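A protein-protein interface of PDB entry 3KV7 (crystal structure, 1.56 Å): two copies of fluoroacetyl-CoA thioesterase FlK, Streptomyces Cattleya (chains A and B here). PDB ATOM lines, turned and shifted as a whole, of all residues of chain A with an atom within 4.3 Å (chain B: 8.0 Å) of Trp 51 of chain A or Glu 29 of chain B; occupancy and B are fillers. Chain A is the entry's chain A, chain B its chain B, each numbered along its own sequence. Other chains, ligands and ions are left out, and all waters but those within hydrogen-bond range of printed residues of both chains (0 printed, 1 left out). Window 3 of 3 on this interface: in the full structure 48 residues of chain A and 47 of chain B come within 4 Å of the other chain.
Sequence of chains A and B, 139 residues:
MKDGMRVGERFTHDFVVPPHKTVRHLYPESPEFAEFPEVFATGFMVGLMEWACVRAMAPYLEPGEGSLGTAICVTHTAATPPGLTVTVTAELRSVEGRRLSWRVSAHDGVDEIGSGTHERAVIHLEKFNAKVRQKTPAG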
ATOM      1  N   HIS A  13     -18.898  23.375 -19.387  1.00  0.00           N
ATOM      2  CA  HIS A  13     -17.581  23.892 -19.302  1.00  0.00           C
ATOM      3  C   HIS A  13     -17.624  25.424 -19.442  1.00  0.00           C
ATOM      4  O   HIS A  13     -18.164  25.878 -20.454  1.00  0.00           O
ATOM      5  CB  HIS A  13     -16.807  23.223 -20.494  1.00  0.00           C
ATOM      6  CG  HIS A  13     -15.452  23.718 -20.651  1.00  0.00           C
ATOM      7  ND1 HIS A  13     -14.437  23.205 -19.886  1.00  0.00           N
ATOM      8  CD2 HIS A  13     -14.877  24.578 -21.534  1.00  0.00           C
ATOM      9  CE1 HIS A  13     -13.293  23.808 -20.212  1.00  0.00           C
ATOM     10  NE2 HIS A  13     -13.527  24.631 -21.219  1.00  0.00           N
ATOM     11  N   PHE A  15     -15.772  29.375 -19.593  1.00  0.00           N
ATOM     12  CA  PHE A  15     -14.527  30.005 -19.932  1.00  0.00           C
ATOM     13  C   PHE A  15     -14.676  31.476 -20.170  1.00  0.00           C
ATOM     14  O   PHE A  15     -15.407  31.933 -21.065  1.00  0.00           O
ATOM     15  CB  PHE A  15     -14.067  29.356 -21.309  1.00  0.00           C
ATOM     16  CG  PHE A  15     -12.777  29.879 -21.839  1.00  0.00           C
ATOM     17  CD1 PHE A  15     -11.524  29.519 -21.233  1.00  0.00           C
ATOM     18  CD2 PHE A  15     -12.757  30.767 -22.935  1.00  0.00           C
ATOM     19  CE1 PHE A  15     -10.285  30.046 -21.711  1.00  0.00           C
ATOM     20  CE2 PHE A  15     -11.524  31.275 -23.394  1.00  0.00           C
ATOM     21  CZ  PHE A  15     -10.290  30.946 -22.798  1.00  0.00           C
ATOM     22  N   HIS A  20      -6.848  37.493 -25.891  1.00  0.00           N
ATOM     23  CA  HIS A  20      -5.992  36.806 -26.865  1.00  0.00           C
ATOM     24  C   HIS A  20      -6.718  35.615 -27.526  1.00  0.00           C
ATOM     25  O   HIS A  20      -6.088  34.724 -28.143  1.00  0.00           O
ATOM     26  CB  HIS A  20      -4.669  36.348 -26.199  1.00  0.00           C
ATOM     27  CG  HIS A  20      -4.846  35.556 -24.919  1.00  0.00           C
ATOM     28  ND1 HIS A  20      -4.923  34.178 -24.905  1.00  0.00           N
ATOM     29  CD2 HIS A  20      -4.988  35.945 -23.623  1.00  0.00           C
ATOM     30  CE1 HIS A  20      -5.111  33.741 -23.671  1.00  0.00           C
ATOM     31  NE2 HIS A  20      -5.110  34.802 -22.864  1.00  0.00           N
ATOM     32  N   LYS A  21      -8.065  35.642 -27.410  1.00  0.00           N
ATOM     33  CA  LYS A  21      -8.898  34.665 -28.150  1.00  0.00           C
ATOM     34  C   LYS A  21      -9.768  35.324 -29.222  1.00  0.00           C
ATOM     35  O   LYS A  21     -10.840  34.826 -29.690  1.00  0.00           O
ATOM     36  CB  LYS A  21      -9.759  33.776 -27.214  1.00  0.00           C
ATOM     37  CG  LYS A  21      -8.997  32.869 -26.284  1.00  0.00           C
ATOM     38  CD  LYS A  21      -8.087  31.934 -26.949  1.00  0.00           C
ATOM     39  CE  LYS A  21      -7.505  31.048 -25.854  1.00  0.00           C
ATOM     40  NZ  LYS A  21      -6.433  30.254 -26.258  1.00  0.00           N
ATOM     41  N   GLY A  47     -12.614  25.188 -30.754  1.00  0.00           N
ATOM     42  CA  GLY A  47     -11.646  24.499 -29.903  1.00  0.00           C
ATOM     43  C   GLY A  47     -12.228  24.422 -28.479  1.00  0.00           C
ATOM     44  O   GLY A  47     -12.013  23.392 -27.824  1.00  0.00           O
ATOM     45  N   LEU A  48     -12.975  25.427 -28.039  1.00  0.00           N
ATOM     46  CA  LEU A  48     -13.606  25.316 -26.716  1.00  0.00           C
ATOM     47  C   LEU A  48     -14.694  24.212 -26.649  1.00  0.00           C
ATOM     48  O   LEU A  48     -14.825  23.532 -25.622  1.00  0.00           O
ATOM     49  CB  LEU A  48     -14.167  26.641 -26.299  1.00  0.00           C
ATOM     50  CG  LEU A  48     -14.785  26.776 -24.909  1.00  0.00           C
ATOM     51  CD1 LEU A  48     -13.633  26.753 -23.965  1.00  0.00           C
ATOM     52  CD2 LEU A  48     -15.475  28.152 -24.799  1.00  0.00           C
ATOM     53  N   MET A  49     -15.449  24.057 -27.729  1.00  0.00           N
ATOM     54  CA  MET A  49     -16.449  23.003 -27.746  1.00  0.00           C
ATOM     55  C   MET A  49     -15.734  21.663 -27.735  1.00  0.00           C
ATOM     56  O   MET A  49     -16.172  20.730 -27.076  1.00  0.00           O
ATOM     57  CB  MET A  49     -17.281  23.187 -29.039  1.00  0.00           C
ATOM     58  CG  MET A  49     -18.254  24.397 -28.941  1.00  0.00           C
ATOM     59  SD  MET A  49     -18.947  24.634 -30.642  1.00  0.00           S
ATOM     60  CE  MET A  49     -20.426  25.598 -30.268  1.00  0.00           C
ATOM     61  N   GLU A  50     -14.682  21.509 -28.523  1.00  0.00           N
ATOM     62  CA  GLU A  50     -13.944  20.233 -28.507  1.00  0.00           C
ATOM     63  C   GLU A  50     -13.355  20.003 -27.102  1.00  0.00           C
ATOM     64  O   GLU A  50     -13.401  18.837 -26.665  1.00  0.00           O
ATOM     65  CB  GLU A  50     -12.905  20.200 -29.661  1.00  0.00           C
ATOM     66  CG  GLU A  50     -13.617  20.347 -30.956  1.00  0.00           C
ATOM     67  CD  GLU A  50     -12.794  20.224 -32.270  1.00  0.00           C
ATOM     68  OE1 GLU A  50     -11.549  20.148 -32.184  1.00  0.00           O
ATOM     69  OE2 GLU A  50     -13.479  20.142 -33.374  1.00  0.00           O
ATOM     70  N   TRP A  51     -12.782  21.018 -26.497  1.00  0.00           N
ATOM     71  CA  TRP A  51     -12.221  20.846 -25.126  1.00  0.00           C
ATOM     72  C   TRP A  51     -13.302  20.333 -24.151  1.00  0.00           C
ATOM     73  O   TRP A  51     -13.006  19.412 -23.346  1.00  0.00           O
ATOM     74  CB  TRP A  51     -11.688  22.195 -24.699  1.00  0.00           C
ATOM     75  CG  TRP A  51     -10.951  22.229 -23.374  1.00  0.00           C
ATOM     76  CD1 TRP A  51     -10.562  21.174 -22.602  1.00  0.00           C
ATOM     77  CD2 TRP A  51     -10.489  23.424 -22.746  1.00  0.00           C
ATOM     78  NE1 TRP A  51      -9.910  21.692 -21.471  1.00  0.00           N
ATOM     79  CE2 TRP A  51      -9.836  23.043 -21.536  1.00  0.00           C
ATOM     80  CE3 TRP A  51     -10.542  24.778 -23.071  1.00  0.00           C
ATOM     81  CZ2 TRP A  51      -9.298  23.991 -20.666  1.00  0.00           C
ATOM     82  CZ3 TRP A  51     -10.007  25.724 -22.198  1.00  0.00           C
ATOM     83  CH2 TRP A  51      -9.400  25.316 -20.998  1.00  0.00           C
ATOM     84  N   ALA A  52     -14.513  20.875 -24.244  1.00  0.00           N
ATOM     85  CA  ALA A  52     -15.641  20.406 -23.370  1.00  0.00           C
ATOM     86  C   ALA A  52     -15.875  18.895 -23.588  1.00  0.00           C
ATOM     87  O   ALA A  52     -16.026  18.100 -22.643  1.00  0.00           O
ATOM     88  CB  ALA A  52     -16.914  21.128 -23.587  1.00  0.00           C
ATOM     89  N   CYS A  53     -15.858  18.439 -24.863  1.00  0.00           N
ATOM     90  CA  CYS A  53     -16.158  17.035 -25.174  1.00  0.00           C
ATOM     91  C   CYS A  53     -15.004  16.109 -24.742  1.00  0.00           C
ATOM     92  O   CYS A  53     -15.215  14.989 -24.277  1.00  0.00           O
ATOM     93  CB  CYS A  53     -16.355  16.848 -26.705  1.00  0.00           C
ATOM     94  SG  CYS A  53     -17.936  17.658 -27.199  1.00  0.00           S
ATOM     95  N   VAL A  54     -13.752  16.602 -24.903  1.00  0.00           N
ATOM     96  CA  VAL A  54     -12.585  15.811 -24.443  1.00  0.00           C
ATOM     97  C   VAL A  54     -12.697  15.614 -22.911  1.00  0.00           C
ATOM     98  O   VAL A  54     -12.409  14.494 -22.453  1.00  0.00           O
ATOM     99  CB  VAL A  54     -11.312  16.631 -24.790  1.00  0.00           C
ATOM    100  CG1 VAL A  54     -10.057  16.114 -23.979  1.00  0.00           C
ATOM    101  CG2 VAL A  54     -10.965  16.533 -26.310  1.00  0.00           C
ATOM    102  N   ARG A  55     -13.066  16.660 -22.178  1.00  0.00           N
ATOM    103  CA  ARG A  55     -13.167  16.539 -20.691  1.00  0.00           C
ATOM    104  C   ARG A  55     -14.323  15.556 -20.379  1.00  0.00           C
ATOM    105  O   ARG A  55     -14.184  14.681 -19.476  1.00  0.00           O
ATOM    106  CB  ARG A  55     -13.431  17.866 -20.032  1.00  0.00           C
ATOM    107  CG  ARG A  55     -12.127  18.689 -20.007  1.00  0.00           C
ATOM    108  CD  ARG A  55     -12.377  19.965 -19.388  1.00  0.00           C
ATOM    109  NE  ARG A  55     -12.630  19.858 -17.930  1.00  0.00           N
ATOM    110  CZ  ARG A  55     -13.064  20.809 -17.193  1.00  0.00           C
ATOM    111  NH1 ARG A  55     -13.501  21.950 -17.737  1.00  0.00           N
ATOM    112  NH2 ARG A  55     -13.054  20.640 -15.826  1.00  0.00           N
ATOM    113  N   ARG B  24      -1.958  21.924 -28.997  1.00  0.00           N
ATOM    114  CA  ARG B  24      -1.606  22.645 -27.731  1.00  0.00           C
ATOM    115  C   ARG B  24      -1.558  24.178 -27.738  1.00  0.00           C
ATOM    116  O   ARG B  24      -1.761  24.871 -26.694  1.00  0.00           O
ATOM    117  CB  ARG B  24      -0.274  22.095 -27.123  1.00  0.00           C
ATOM    118  CG  ARG B  24       0.940  22.307 -27.991  1.00  0.00           C
ATOM    119  CD  ARG B  24       2.161  21.636 -27.298  1.00  0.00           C
ATOM    120  NE  ARG B  24       3.378  21.898 -28.043  1.00  0.00           N
ATOM    121  CZ  ARG B  24       4.292  22.860 -27.844  1.00  0.00           C
ATOM    122  NH1 ARG B  24       4.162  23.780 -26.893  1.00  0.00           N
ATOM    123  NH2 ARG B  24       5.364  22.892 -28.654  1.00  0.00           N
ATOM    124  N   HIS B  25      -1.332  24.710 -28.962  1.00  0.00           N
ATOM    125  CA  HIS B  25      -1.236  26.138 -29.137  1.00  0.00           C
ATOM    126  C   HIS B  25      -2.596  26.796 -29.266  1.00  0.00           C
ATOM    127  O   HIS B  25      -2.725  28.047 -29.121  1.00  0.00           O
ATOM    128  CB  HIS B  25      -0.393  26.403 -30.394  1.00  0.00           C
ATOM    129  CG  HIS B  25       1.027  26.079 -30.221  1.00  0.00           C
ATOM    130  ND1 HIS B  25       1.915  27.001 -29.714  1.00  0.00           N
ATOM    131  CD2 HIS B  25       1.704  24.952 -30.495  1.00  0.00           C
ATOM    132  CE1 HIS B  25       3.113  26.417 -29.652  1.00  0.00           C
ATOM    133  NE2 HIS B  25       3.018  25.188 -30.113  1.00  0.00           N
ATOM    134  N   LEU B  26      -3.619  25.999 -29.603  1.00  0.00           N
ATOM    135  CA  LEU B  26      -4.961  26.615 -29.676  1.00  0.00           C
ATOM    136  C   LEU B  26      -5.505  27.051 -28.327  1.00  0.00           C
ATOM    137  O   LEU B  26      -6.120  28.134 -28.202  1.00  0.00           O
ATOM    138  CB  LEU B  26      -5.910  25.642 -30.440  1.00  0.00           C
ATOM    139  CG  LEU B  26      -7.313  26.201 -30.756  1.00  0.00           C
ATOM    140  CD1 LEU B  26      -7.218  27.166 -31.929  1.00  0.00           C
ATOM    141  CD2 LEU B  26      -8.186  25.037 -31.193  1.00  0.00           C
ATOM    142  N   TYR B  27      -5.261  26.201 -27.345  1.00  0.00           N
ATOM    143  CA  TYR B  27      -5.564  26.563 -25.932  1.00  0.00           C
ATOM    144  C   TYR B  27      -4.411  26.198 -25.043  1.00  0.00           C
ATOM    145  O   TYR B  27      -4.424  25.142 -24.488  1.00  0.00           O
ATOM    146  CB  TYR B  27      -6.848  25.854 -25.446  1.00  0.00           C
ATOM    147  CG  TYR B  27      -8.058  26.618 -25.859  1.00  0.00           C
ATOM    148  CD1 TYR B  27      -8.646  27.600 -25.038  1.00  0.00           C
ATOM    149  CD2 TYR B  27      -8.694  26.339 -27.142  1.00  0.00           C
ATOM    150  CE1 TYR B  27      -9.748  28.318 -25.429  1.00  0.00           C
ATOM    151  CE2 TYR B  27      -9.849  27.023 -27.536  1.00  0.00           C
ATOM    152  CZ  TYR B  27     -10.405  28.022 -26.724  1.00  0.00           C
ATOM    153  OH  TYR B  27     -11.503  28.779 -27.088  1.00  0.00           O
ATOM    154  N   PRO B  28      -3.447  27.118 -24.925  1.00  0.00           N
ATOM    155  CA  PRO B  28      -2.316  26.897 -23.961  1.00  0.00           C
ATOM    156  C   PRO B  28      -2.865  26.752 -22.539  1.00  0.00           C
ATOM    157  O   PRO B  28      -2.166  26.146 -21.724  1.00  0.00           O
ATOM    158  CB  PRO B  28      -1.499  28.182 -24.077  1.00  0.00           C
ATOM    159  CG  PRO B  28      -1.719  28.595 -25.596  1.00  0.00           C
ATOM    160  CD  PRO B  28      -3.311  28.405 -25.659  1.00  0.00           C
ATOM    161  N   GLU B  29      -4.046  27.296 -22.217  1.00  0.00           N
ATOM    162  CA  GLU B  29      -4.582  27.118 -20.880  1.00  0.00           C
ATOM    163  C   GLU B  29      -5.244  25.771 -20.640  1.00  0.00           C
ATOM    164  O   GLU B  29      -5.763  25.543 -19.544  1.00  0.00           O
ATOM    165  CB  GLU B  29      -5.557  28.207 -20.561  1.00  0.00           C
ATOM    166  CG  GLU B  29      -6.691  28.389 -21.465  1.00  0.00           C
ATOM    167  CD  GLU B  29      -6.368  29.435 -22.645  1.00  0.00           C
ATOM    168  OE1 GLU B  29      -6.824  30.603 -22.586  1.00  0.00           O
ATOM    169  OE2 GLU B  29      -5.727  29.026 -23.655  1.00  0.00           O
ATOM    170  N   SER B  30      -5.222  24.859 -21.618  1.00  0.00           N
ATOM    171  CA  SER B  30      -5.886  23.538 -21.451  1.00  0.00           C
ATOM    172  C   SER B  30      -4.848  22.516 -21.176  1.00  0.00           C
ATOM    173  O   SER B  30      -4.002  22.184 -22.030  1.00  0.00           O
ATOM    174  CB  SER B  30      -6.663  23.138 -22.760  1.00  0.00           C
ATOM    175  OG  SER B  30      -6.958  21.734 -22.658  1.00  0.00           O
ATOM    176  N   PRO B  31      -4.845  21.961 -19.956  1.00  0.00           N
ATOM    177  CA  PRO B  31      -3.976  20.844 -19.715  1.00  0.00           C
ATOM    178  C   PRO B  31      -4.215  19.608 -20.550  1.00  0.00           C
ATOM    179  O   PRO B  31      -3.296  18.844 -20.799  1.00  0.00           O
ATOM    180  CB  PRO B  31      -4.126  20.560 -18.170  1.00  0.00           C
ATOM    181  CG  PRO B  31      -4.813  21.823 -17.623  1.00  0.00           C
ATOM    182  CD  PRO B  31      -5.701  22.316 -18.813  1.00  0.00           C
ATOM    183  N   GLU B  32      -5.468  19.460 -20.970  1.00  0.00           N
ATOM    184  CA  GLU B  32      -5.807  18.329 -21.803  1.00  0.00           C
ATOM    185  C   GLU B  32      -5.079  18.486 -23.154  1.00  0.00           C
ATOM    186  O   GLU B  32      -4.442  17.532 -23.610  1.00  0.00           O
ATOM    187  CB  GLU B  32      -7.350  18.171 -22.049  1.00  0.00           C
ATOM    188  CG  GLU B  32      -8.066  17.667 -20.788  1.00  0.00           C
ATOM    189  CD  GLU B  32      -8.372  18.728 -19.736  1.00  0.00           C
ATOM    190  OE1 GLU B  32      -8.770  18.269 -18.669  1.00  0.00           O
ATOM    191  OE2 GLU B  32      -8.240  19.954 -19.945  1.00  0.00           O
ATOM    192  N   PHE B  33      -5.164  19.662 -23.715  1.00  0.00           N
ATOM    193  CA  PHE B  33      -4.612  19.882 -25.074  1.00  0.00           C
ATOM    194  C   PHE B  33      -3.085  19.868 -25.016  1.00  0.00           C
ATOM    195  O   PHE B  33      -2.425  19.517 -26.048  1.00  0.00           O
ATOM    196  CB  PHE B  33      -5.077  21.214 -25.690  1.00  0.00           C
ATOM    197  CG  PHE B  33      -6.487  21.210 -26.183  1.00  0.00           C
ATOM    198  CD1 PHE B  33      -6.976  22.337 -26.828  1.00  0.00           C
ATOM    199  CD2 PHE B  33      -7.281  20.086 -26.077  1.00  0.00           C
ATOM    200  CE1 PHE B  33      -8.298  22.385 -27.351  1.00  0.00           C
ATOM    201  CE2 PHE B  33      -8.594  20.136 -26.582  1.00  0.00           C
ATOM    202  CZ  PHE B  33      -9.137  21.286 -27.096  1.00  0.00           C
ATOM    203  N   ALA B  34      -2.525  20.129 -23.818  1.00  0.00           N
ATOM    204  CA  ALA B  34      -1.043  20.227 -23.715  1.00  0.00           C
ATOM    205  C   ALA B  34      -0.350  18.906 -24.015  1.00  0.00           C
ATOM    206  O   ALA B  34       0.814  18.941 -24.382  1.00  0.00           O
ATOM    207  CB  ALA B  34      -0.671  20.775 -22.295  1.00  0.00           C
ATOM    208  N   PHE B  36      -1.656  16.600 -26.254  1.00  0.00           N
ATOM    209  CA  PHE B  36      -2.105  16.053 -27.522  1.00  0.00           C
ATOM    210  C   PHE B  36      -0.939  15.852 -28.549  1.00  0.00           C
ATOM    211  O   PHE B  36       0.065  16.542 -28.471  1.00  0.00           O
ATOM    212  CB  PHE B  36      -3.174  17.012 -28.156  1.00  0.00           C
ATOM    213  CG  PHE B  36      -4.621  16.597 -27.902  1.00  0.00           C
ATOM    214  CD1 PHE B  36      -5.505  16.350 -28.978  1.00  0.00           C
ATOM    215  CD2 PHE B  36      -5.076  16.427 -26.595  1.00  0.00           C
ATOM    216  CE1 PHE B  36      -6.858  16.013 -28.665  1.00  0.00           C
ATOM    217  CE2 PHE B  36      -6.370  16.060 -26.315  1.00  0.00           C
ATOM    218  CZ  PHE B  36      -7.255  15.866 -27.341  1.00  0.00           C
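Printed residues of chain B that touch a printed residue of chain A: Leu 26, Tyr 27, Pro 28, Glu 29, Ser 30, Glu 32, Phe 33 and Phe 36. Hydrophobic or aromatic side chains of chain B that line the printed part of chain A: Leu 26, Tyr 27, Pro 28, Phe 33 and Phe 36. Among the printed residues, 19 pairs touch across the chains. Among the printed residues, Asp or Glu carboxylates within 4 Å of a Lys or Arg side-chain nitrogen of the other chain: Lys 21 of chain A with Glu 29 of chain B.
No position is printed for both chains. Of the 19 pairs that touch across the chains among the printed residues, none has its exchanged pair printed and touching as well.
ND1 of His 13 of chain A sits at hydrogen-bond distance from NH1 of Arg 55 of chain A. The side-chain hydroxyl of Ser 30 of chain B lies within hydrogen-bond range of the backbone NH of Phe 33 of chain B (2.9 Å). The side-chain hydroxyl (OG) of Ser 30 of chain B sits close to the backbone NH (N) of Glu 32 of chain B.
Printed residues of chain B within 4 Å of His 20 of chain A: Glu 29 (3.7 Å). Printed residues of chain B within 4 Å of Lys 21 of chain A: Leu 26 (2.9 Å), Tyr 27 (3.6 Å), Pro 28 (3.7 Å) and Glu 29 (3.0 Å). Of chain B, only Tyr 27 (3.7 Å), Glu 29 (3.9 Å), Ser 30 (3.2 Å), Glu 32 (2.9 Å) and Phe 33 (3.6 Å) come within 4 Å of Trp 51 of chain A. No residue of chain B comes within 4 Å of Ala 52 of chain A. Of the printed residues of chain A, Tyr 27 of chain B touches Phe 15, Lys 21, Gly 47, Leu 48 and Trp 51. Glu 29 of chain B touches four residues of chain A. The nearest printed residue of chain A that does not touch Glu 29 of chain B is Leu 48 of chain A (7.6 Å). The nearest printed residue of chain A that does not touch Ser 30 of chain B is Val 54 of chain A (6.6 Å).
Among the printed residues, pairs that only touch across the chains: Phe 15 of chain A with Tyr 27 of chain B, Phe 15 of chain A with Glu 29 of chain B, His 20 of chain A with Glu 29 of chain B, Lys 21 of chain A with Tyr 27 of chain B, Lys 21 of chain A with Pro 28 of chain B, Gly 47 of chain A with Leu 26 of chain B, Gly 47 of chain A with Tyr 27 of chain B, Gly 47 of chain A with Phe 33 of chain B, Leu 48 of chain A with Tyr 27 of chain B, Trp 51 of chain A with Tyr 27 of chain B, Trp 51 of chain A with Glu 29 of chain B, Trp 51 of chain A with Phe 33 of chain B, Val 54 of chain A with Glu 32 of chain B, Val 54 of chain A with Phe 36 of chain B and Arg 55 of chain A with Glu 32 of chain B.
NE1 of Trp 51 of chain A lies within hydrogen-bond range of OG of Ser 30 of chain B (3.2 Å). The indole nitrogen (NE1) of Trp 51 of chain A sits at hydrogen-bond distance from the side-chain carboxylate (OE2) of Glu 32 of chain B (2.9 Å). O of Leu 26 of chain B is in hydrogen-bond range of NZ of Lys 21 of chain A, 2.9 Å away. NZ of Lys 21 of chain A is in salt-bridge range of OE2 of Glu 29 of chain B.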
